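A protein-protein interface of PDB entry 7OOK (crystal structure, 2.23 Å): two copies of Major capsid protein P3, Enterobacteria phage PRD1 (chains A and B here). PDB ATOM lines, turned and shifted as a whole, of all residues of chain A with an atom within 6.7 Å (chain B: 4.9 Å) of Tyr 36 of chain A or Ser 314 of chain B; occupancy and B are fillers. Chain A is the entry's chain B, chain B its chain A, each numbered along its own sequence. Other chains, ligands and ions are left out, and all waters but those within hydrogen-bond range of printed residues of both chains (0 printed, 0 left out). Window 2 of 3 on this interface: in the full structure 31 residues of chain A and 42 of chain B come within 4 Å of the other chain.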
ATOM      1  N   VAL A  31     -15.755   9.432  -0.495  1.00  0.00           N
ATOM      2  CA  VAL A  31     -16.112   9.257   0.911  1.00  0.00           C
ATOM      3  C   VAL A  31     -16.026   7.786   1.301  1.00  0.00           C
ATOM      4  O   VAL A  31     -15.466   7.435   2.346  1.00  0.00           O
ATOM      5  CB  VAL A  31     -17.516   9.829   1.183  1.00  0.00           C
ATOM      6  CG1 VAL A  31     -18.014   9.403   2.557  1.00  0.00           C
ATOM      7  CG2 VAL A  31     -17.495  11.342   1.078  1.00  0.00           C
ATOM      8  N   LEU A  32     -16.586   6.905   0.471  1.00  0.00           N
ATOM      9  CA  LEU A  32     -16.576   5.484   0.799  1.00  0.00           C
ATOM     10  C   LEU A  32     -15.160   4.922   0.833  1.00  0.00           C
ATOM     11  O   LEU A  32     -14.871   4.022   1.631  1.00  0.00           O
ATOM     12  CB  LEU A  32     -17.434   4.709  -0.201  1.00  0.00           C
ATOM     13  CG  LEU A  32     -18.942   4.953  -0.104  1.00  0.00           C
ATOM     14  CD1 LEU A  32     -19.659   4.263  -1.250  1.00  0.00           C
ATOM     15  CD2 LEU A  32     -19.490   4.474   1.235  1.00  0.00           C
ATOM     16  N   GLN A  33     -14.262   5.436  -0.013  1.00  0.00           N
ATOM     17  CA  GLN A  33     -12.892   4.935  -0.021  1.00  0.00           C
ATOM     18  C   GLN A  33     -12.095   5.459   1.166  1.00  0.00           C
ATOM     19  O   GLN A  33     -11.316   4.715   1.774  1.00  0.00           O
ATOM     20  CB  GLN A  33     -12.187   5.325  -1.323  1.00  0.00           C
ATOM     21  CG  GLN A  33     -10.770   4.766  -1.446  1.00  0.00           C
ATOM     22  CD  GLN A  33      -9.935   5.488  -2.489  1.00  0.00           C
ATOM     23  OE1 GLN A  33     -10.359   6.499  -3.052  1.00  0.00           O
ATOM     24  NE2 GLN A  33      -8.737   4.973  -2.747  1.00  0.00           N
ATOM     25  N   GLN A  34     -12.274   6.734   1.506  1.00  0.00           N
ATOM     26  CA  GLN A  34     -11.427   7.387   2.493  1.00  0.00           C
ATOM     27  C   GLN A  34     -12.002   7.347   3.901  1.00  0.00           C
ATOM     28  O   GLN A  34     -11.240   7.410   4.873  1.00  0.00           O
ATOM     29  CB  GLN A  34     -11.197   8.849   2.094  1.00  0.00           C
ATOM     30  CG  GLN A  34     -10.655   9.039   0.684  1.00  0.00           C
ATOM     31  CD  GLN A  34      -9.232   8.539   0.533  1.00  0.00           C
ATOM     32  OE1 GLN A  34      -8.400   8.722   1.422  1.00  0.00           O
ATOM     33  NE2 GLN A  34      -8.949   7.898  -0.594  1.00  0.00           N
ATOM     34  N   SER A  35     -13.321   7.245   4.040  1.00  0.00           N
ATOM     35  CA  SER A  35     -13.935   7.421   5.345  1.00  0.00           C
ATOM     36  C   SER A  35     -13.711   6.194   6.228  1.00  0.00           C
ATOM     37  O   SER A  35     -13.223   5.149   5.790  1.00  0.00           O
ATOM     38  CB  SER A  35     -15.430   7.707   5.204  1.00  0.00           C
ATOM     39  OG  SER A  35     -16.111   6.604   4.633  1.00  0.00           O
ATOM     40  N   TYR A  36     -14.097   6.339   7.494  1.00  0.00           N
ATOM     41  CA  TYR A  36     -13.852   5.357   8.544  1.00  0.00           C
ATOM     42  C   TYR A  36     -15.176   4.735   8.977  1.00  0.00           C
ATOM     43  O   TYR A  36     -15.929   5.356   9.741  1.00  0.00           O
ATOM     44  CB  TYR A  36     -13.162   6.056   9.724  1.00  0.00           C
ATOM     45  CG  TYR A  36     -12.501   5.159  10.741  1.00  0.00           C
ATOM     46  CD1 TYR A  36     -11.455   4.320  10.385  1.00  0.00           C
ATOM     47  CD2 TYR A  36     -12.901   5.184  12.072  1.00  0.00           C
ATOM     48  CE1 TYR A  36     -10.841   3.509  11.321  1.00  0.00           C
ATOM     49  CE2 TYR A  36     -12.296   4.378  13.014  1.00  0.00           C
ATOM     50  CZ  TYR A  36     -11.265   3.544  12.635  1.00  0.00           C
ATOM     51  OH  TYR A  36     -10.659   2.741  13.575  1.00  0.00           O
ATOM     52  N   PRO A  37     -15.516   3.527   8.517  1.00  0.00           N
ATOM     53  CA  PRO A  37     -16.818   2.940   8.880  1.00  0.00           C
ATOM     54  C   PRO A  37     -16.822   2.447  10.319  1.00  0.00           C
ATOM     55  O   PRO A  37     -15.928   1.711  10.740  1.00  0.00           O
ATOM     56  CB  PRO A  37     -16.977   1.785   7.885  1.00  0.00           C
ATOM     57  CG  PRO A  37     -15.576   1.376   7.579  1.00  0.00           C
ATOM     58  CD  PRO A  37     -14.742   2.639   7.626  1.00  0.00           C
ATOM     59  N   VAL A  38     -17.849   2.845  11.068  1.00  0.00           N
ATOM     60  CA  VAL A  38     -17.949   2.533  12.489  1.00  0.00           C
ATOM     61  C   VAL A  38     -19.379   2.129  12.815  1.00  0.00           C
ATOM     62  O   VAL A  38     -20.336   2.746  12.338  1.00  0.00           O
ATOM     63  CB  VAL A  38     -17.524   3.734  13.361  1.00  0.00           C
ATOM     64  CG1 VAL A  38     -17.729   3.430  14.843  1.00  0.00           C
ATOM     65  CG2 VAL A  38     -16.077   4.110  13.079  1.00  0.00           C
ATOM     66  N   TYR A 236     -22.109   4.683  11.180  1.00  0.00           N
ATOM     67  CA  TYR A 236     -21.776   5.966  10.582  1.00  0.00           C
ATOM     68  C   TYR A 236     -20.377   5.908   9.989  1.00  0.00           C
ATOM     69  O   TYR A 236     -19.646   4.927  10.148  1.00  0.00           O
ATOM     70  CB  TYR A 236     -21.879   7.096  11.611  1.00  0.00           C
ATOM     71  CG  TYR A 236     -20.930   6.944  12.777  1.00  0.00           C
ATOM     72  CD1 TYR A 236     -21.280   6.191  13.892  1.00  0.00           C
ATOM     73  CD2 TYR A 236     -19.685   7.558  12.766  1.00  0.00           C
ATOM     74  CE1 TYR A 236     -20.415   6.056  14.961  1.00  0.00           C
ATOM     75  CE2 TYR A 236     -18.813   7.427  13.829  1.00  0.00           C
ATOM     76  CZ  TYR A 236     -19.184   6.675  14.924  1.00  0.00           C
ATOM     77  OH  TYR A 236     -18.321   6.542  15.986  1.00  0.00           O
ATOM     78  N   LEU A 237     -20.013   6.983   9.295  1.00  0.00           N
ATOM     79  CA  LEU A 237     -18.696   7.133   8.688  1.00  0.00           C
ATOM     80  C   LEU A 237     -17.946   8.252   9.399  1.00  0.00           C
ATOM     81  O   LEU A 237     -18.443   9.382   9.483  1.00  0.00           O
ATOM     82  CB  LEU A 237     -18.806   7.439   7.197  1.00  0.00           C
ATOM     83  CG  LEU A 237     -19.544   6.406   6.348  1.00  0.00           C
ATOM     84  CD1 LEU A 237     -19.725   6.916   4.928  1.00  0.00           C
ATOM     85  CD2 LEU A 237     -18.804   5.077   6.343  1.00  0.00           C
ATOM     86  N   ASP A 238     -16.757   7.939   9.895  1.00  0.00           N
ATOM     87  CA  ASP A 238     -15.878   8.908  10.531  1.00  0.00           C
ATOM     88  C   ASP A 238     -14.699   9.203   9.612  1.00  0.00           C
ATOM     89  O   ASP A 238     -14.496   8.545   8.586  1.00  0.00           O
ATOM     90  CB  ASP A 238     -15.392   8.383  11.888  1.00  0.00           C
ATOM     91  CG  ASP A 238     -15.318   9.471  12.946  1.00  0.00           C
ATOM     92  OD1 ASP A 238     -15.558  10.653  12.619  1.00  0.00           O
ATOM     93  OD2 ASP A 238     -15.022   9.140  14.115  1.00  0.00           O
ATOM     94  N   GLN A 239     -13.915  10.212   9.989  1.00  0.00           N
ATOM     95  CA  GLN A 239     -12.706  10.577   9.253  1.00  0.00           C
ATOM     96  C   GLN A 239     -13.035  10.949   7.809  1.00  0.00           C
ATOM     97  O   GLN A 239     -12.454  10.420   6.858  1.00  0.00           O
ATOM     98  CB  GLN A 239     -11.682   9.440   9.288  1.00  0.00           C
ATOM     99  CG  GLN A 239     -11.319   8.955  10.679  1.00  0.00           C
ATOM    100  CD  GLN A 239     -10.405   9.912  11.410  1.00  0.00           C
ATOM    101  OE1 GLN A 239     -10.687  11.107  11.511  1.00  0.00           O
ATOM    102  NE2 GLN A 239      -9.294   9.392  11.922  1.00  0.00           N
ATOM    103  N   LEU A 240     -13.982  11.864   7.647  1.00  0.00           N
ATOM    104  CA  LEU A 240     -14.396  12.258   6.310  1.00  0.00           C
ATOM    105  C   LEU A 240     -13.244  12.960   5.593  1.00  0.00           C
ATOM    106  O   LEU A 240     -12.491  13.716   6.215  1.00  0.00           O
ATOM    107  CB  LEU A 240     -15.614  13.176   6.376  1.00  0.00           C
ATOM    108  CG  LEU A 240     -16.858  12.594   7.050  1.00  0.00           C
ATOM    109  CD1 LEU A 240     -18.001  13.596   6.994  1.00  0.00           C
ATOM    110  CD2 LEU A 240     -17.269  11.277   6.406  1.00  0.00           C
ATOM    111  N   GLN B 308     -12.913  -5.226  16.891  1.00  0.00           N
ATOM    112  CA  GLN B 308     -11.663  -4.859  16.242  1.00  0.00           C
ATOM    113  C   GLN B 308     -11.332  -3.436  16.674  1.00  0.00           C
ATOM    114  O   GLN B 308     -12.195  -2.553  16.614  1.00  0.00           O
ATOM    115  CB  GLN B 308     -11.773  -4.956  14.722  1.00  0.00           C
ATOM    116  CG  GLN B 308     -11.733  -6.378  14.183  1.00  0.00           C
ATOM    117  CD  GLN B 308     -11.836  -6.427  12.668  1.00  0.00           C
ATOM    118  OE1 GLN B 308     -12.579  -5.659  12.061  1.00  0.00           O
ATOM    119  NE2 GLN B 308     -11.081  -7.331  12.049  1.00  0.00           N
ATOM    120  N   ARG B 309     -10.098  -3.217  17.118  1.00  0.00           N
ATOM    121  CA  ARG B 309      -9.710  -1.975  17.770  1.00  0.00           C
ATOM    122  C   ARG B 309      -8.387  -1.471  17.218  1.00  0.00           C
ATOM    123  O   ARG B 309      -7.453  -2.251  17.006  1.00  0.00           O
ATOM    124  CB  ARG B 309      -9.601  -2.184  19.288  1.00  0.00           C
ATOM    125  CG  ARG B 309      -9.004  -1.025  20.062  1.00  0.00           C
ATOM    126  CD  ARG B 309      -8.893  -1.389  21.533  1.00  0.00           C
ATOM    127  NE  ARG B 309     -10.175  -1.831  22.072  1.00  0.00           N
ATOM    128  CZ  ARG B 309     -10.326  -2.493  23.210  1.00  0.00           C
ATOM    129  NH1 ARG B 309      -9.287  -2.828  23.958  1.00  0.00           N
ATOM    130  NH2 ARG B 309     -11.550  -2.833  23.606  1.00  0.00           N
ATOM    131  N   THR B 310      -8.319  -0.163  16.986  1.00  0.00           N
ATOM    132  CA  THR B 310      -7.091   0.503  16.585  1.00  0.00           C
ATOM    133  C   THR B 310      -6.361   1.038  17.814  1.00  0.00           C
ATOM    134  O   THR B 310      -6.949   1.237  18.880  1.00  0.00           O
ATOM    135  CB  THR B 310      -7.377   1.650  15.616  1.00  0.00           C
ATOM    136  OG1 THR B 310      -8.135   2.665  16.287  1.00  0.00           O
ATOM    137  CG2 THR B 310      -8.159   1.154  14.417  1.00  0.00           C
ATOM    138  N   ASN B 312      -5.331   3.844  18.681  1.00  0.00           N
ATOM    139  CA  ASN B 312      -5.765   5.118  19.234  1.00  0.00           C
ATOM    140  C   ASN B 312      -7.023   4.989  20.079  1.00  0.00           C
ATOM    141  O   ASN B 312      -7.709   5.989  20.328  1.00  0.00           O
ATOM    142  CB  ASN B 312      -5.968   6.149  18.118  1.00  0.00           C
ATOM    143  CG  ASN B 312      -7.147   5.821  17.218  1.00  0.00           C
ATOM    144  OD1 ASN B 312      -8.051   5.075  17.596  1.00  0.00           O
ATOM    145  ND2 ASN B 312      -7.145   6.388  16.019  1.00  0.00           N
ATOM    146  N   PHE B 313      -7.355   3.770  20.492  1.00  0.00           N
ATOM    147  CA  PHE B 313      -8.442   3.461  21.414  1.00  0.00           C
ATOM    148  C   PHE B 313      -9.812   3.442  20.750  1.00  0.00           C
ATOM    149  O   PHE B 313     -10.822   3.330  21.462  1.00  0.00           O
ATOM    150  CB  PHE B 313      -8.481   4.454  22.581  1.00  0.00           C
ATOM    151  N   SER B 314      -9.891   3.531  19.427  1.00  0.00           N
ATOM    152  CA  SER B 314     -11.171   3.567  18.732  1.00  0.00           C
ATOM    153  C   SER B 314     -11.649   2.154  18.417  1.00  0.00           C
ATOM    154  O   SER B 314     -10.886   1.332  17.900  1.00  0.00           O
ATOM    155  CB  SER B 314     -11.053   4.382  17.442  1.00  0.00           C
ATOM    156  OG  SER B 314     -12.266   4.352  16.709  1.00  0.00           O
ATOM    157  N   ASP B 315     -12.918   1.885  18.724  1.00  0.00           N
ATOM    158  CA  ASP B 315     -13.553   0.610  18.412  1.00  0.00           C
ATOM    159  C   ASP B 315     -14.406   0.777  17.161  1.00  0.00           C
ATOM    160  O   ASP B 315     -15.374   1.545  17.164  1.00  0.00           O
ATOM    161  CB  ASP B 315     -14.416   0.128  19.577  1.00  0.00           C
ATOM    162  CG  ASP B 315     -13.633  -0.012  20.862  1.00  0.00           C
ATOM    163  OD1 ASP B 315     -13.206   1.027  21.412  1.00  0.00           O
ATOM    164  OD2 ASP B 315     -13.441  -1.161  21.319  1.00  0.00           O
ATOM    165  N   THR B 316     -14.048   0.060  16.097  1.00  0.00           N
ATOM    166  CA  THR B 316     -14.818   0.141  14.865  1.00  0.00           C
ATOM    167  C   THR B 316     -16.047  -0.758  14.884  1.00  0.00           C
ATOM    168  O   THR B 316     -16.977  -0.526  14.104  1.00  0.00           O
ATOM    169  CB  THR B 316     -13.947  -0.226  13.661  1.00  0.00           C
ATOM    170  OG1 THR B 316     -13.520  -1.588  13.774  1.00  0.00           O
ATOM    171  CG2 THR B 316     -12.732   0.681  13.584  1.00  0.00           C
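O of Val 38 of chain A sits at hydrogen-bond distance from N of Tyr 236 of chain A, at 2.9 Å. The backbone carbonyl oxygen (O) of Gln 308 of chain B sits at hydrogen-bond distance from the backbone NH (N) of Thr 316 of chain B, 3.2 Å away. The guanidinium group of Arg 309 of chain B lies within salt-bridge range of the side-chain carboxylate of Asp 315 of chain B (3.4 Å). The side-chain hydroxyl of Thr 310 of chain B sits at hydrogen-bond distance from the side-chain amide oxygen of Asn 312 of chain B (2.7 Å). The side-chain hydroxyl of Thr 310 of chain B lies within hydrogen-bond range of the backbone carbonyl oxygen of Ser 314 of chain B (3.5 Å). OD1 of Asn 312 of chain B lies within hydrogen-bond range of N of Ser 314 of chain B, at 3.0 Å.
Tyr 36 of chain A touches Thr 310 of chain B. Tyr 36 of chain A touches Ser 314 of chain B (CE2 to OG, 3.7 Å). CG2 of Thr 316 of chain B touches OH of Tyr 36 of chain A (2.9 Å). Asp 315 of chain B touches Val 38 of chain A. Val 38 of chain A touches Thr 316 of chain B (CA to O, 3.6 Å).
Tyr 36 of chain A touches just these residues of chain B: Thr 310 (3.1 Å), Ser 314 (3.7 Å) and Thr 316 (2.9 Å). Of the printed residues of chain B, Val 38 of chain A touches Asp 315 and Thr 316. Leu 240 of chain A touches none of the printed residues of chain B. Of the printed residues of chain A, Thr 310 of chain B touches Tyr 36. Asn 312 of chain B touches none of the printed residues of chain A. Ser 314 of chain B touches just one residue of chain A: Tyr 36. Of the printed residues of chain A, Asp 315 of chain B touches Val 38 (3.8 Å). Of the printed residues of chain A, Thr 316 of chain B touches Tyr 36 (2.9 Å) and Val 38 (3.6 Å). The nearest printed residue of chain A that does not touch Thr 316 of chain B is Pro 37 of chain A (4.03 Å).
Of the 13 printed residues of chain A, 2 touch a printed residue of chain B. Printed residues of chain A that touch a printed residue of chain B: Tyr 36 and Val 38. Hydrophobic or aromatic side chains of chain A within 4 Å of the printed part of chain B: Tyr 36 and Val 38. Along chain A the printed residues that touch a printed residue of chain B span positions 36 to 38. Among the printed residues, no Asp or Glu carboxylate lies within 4 Å of a Lys or Arg side-chain nitrogen of the other chain.
No position is printed for both chains.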
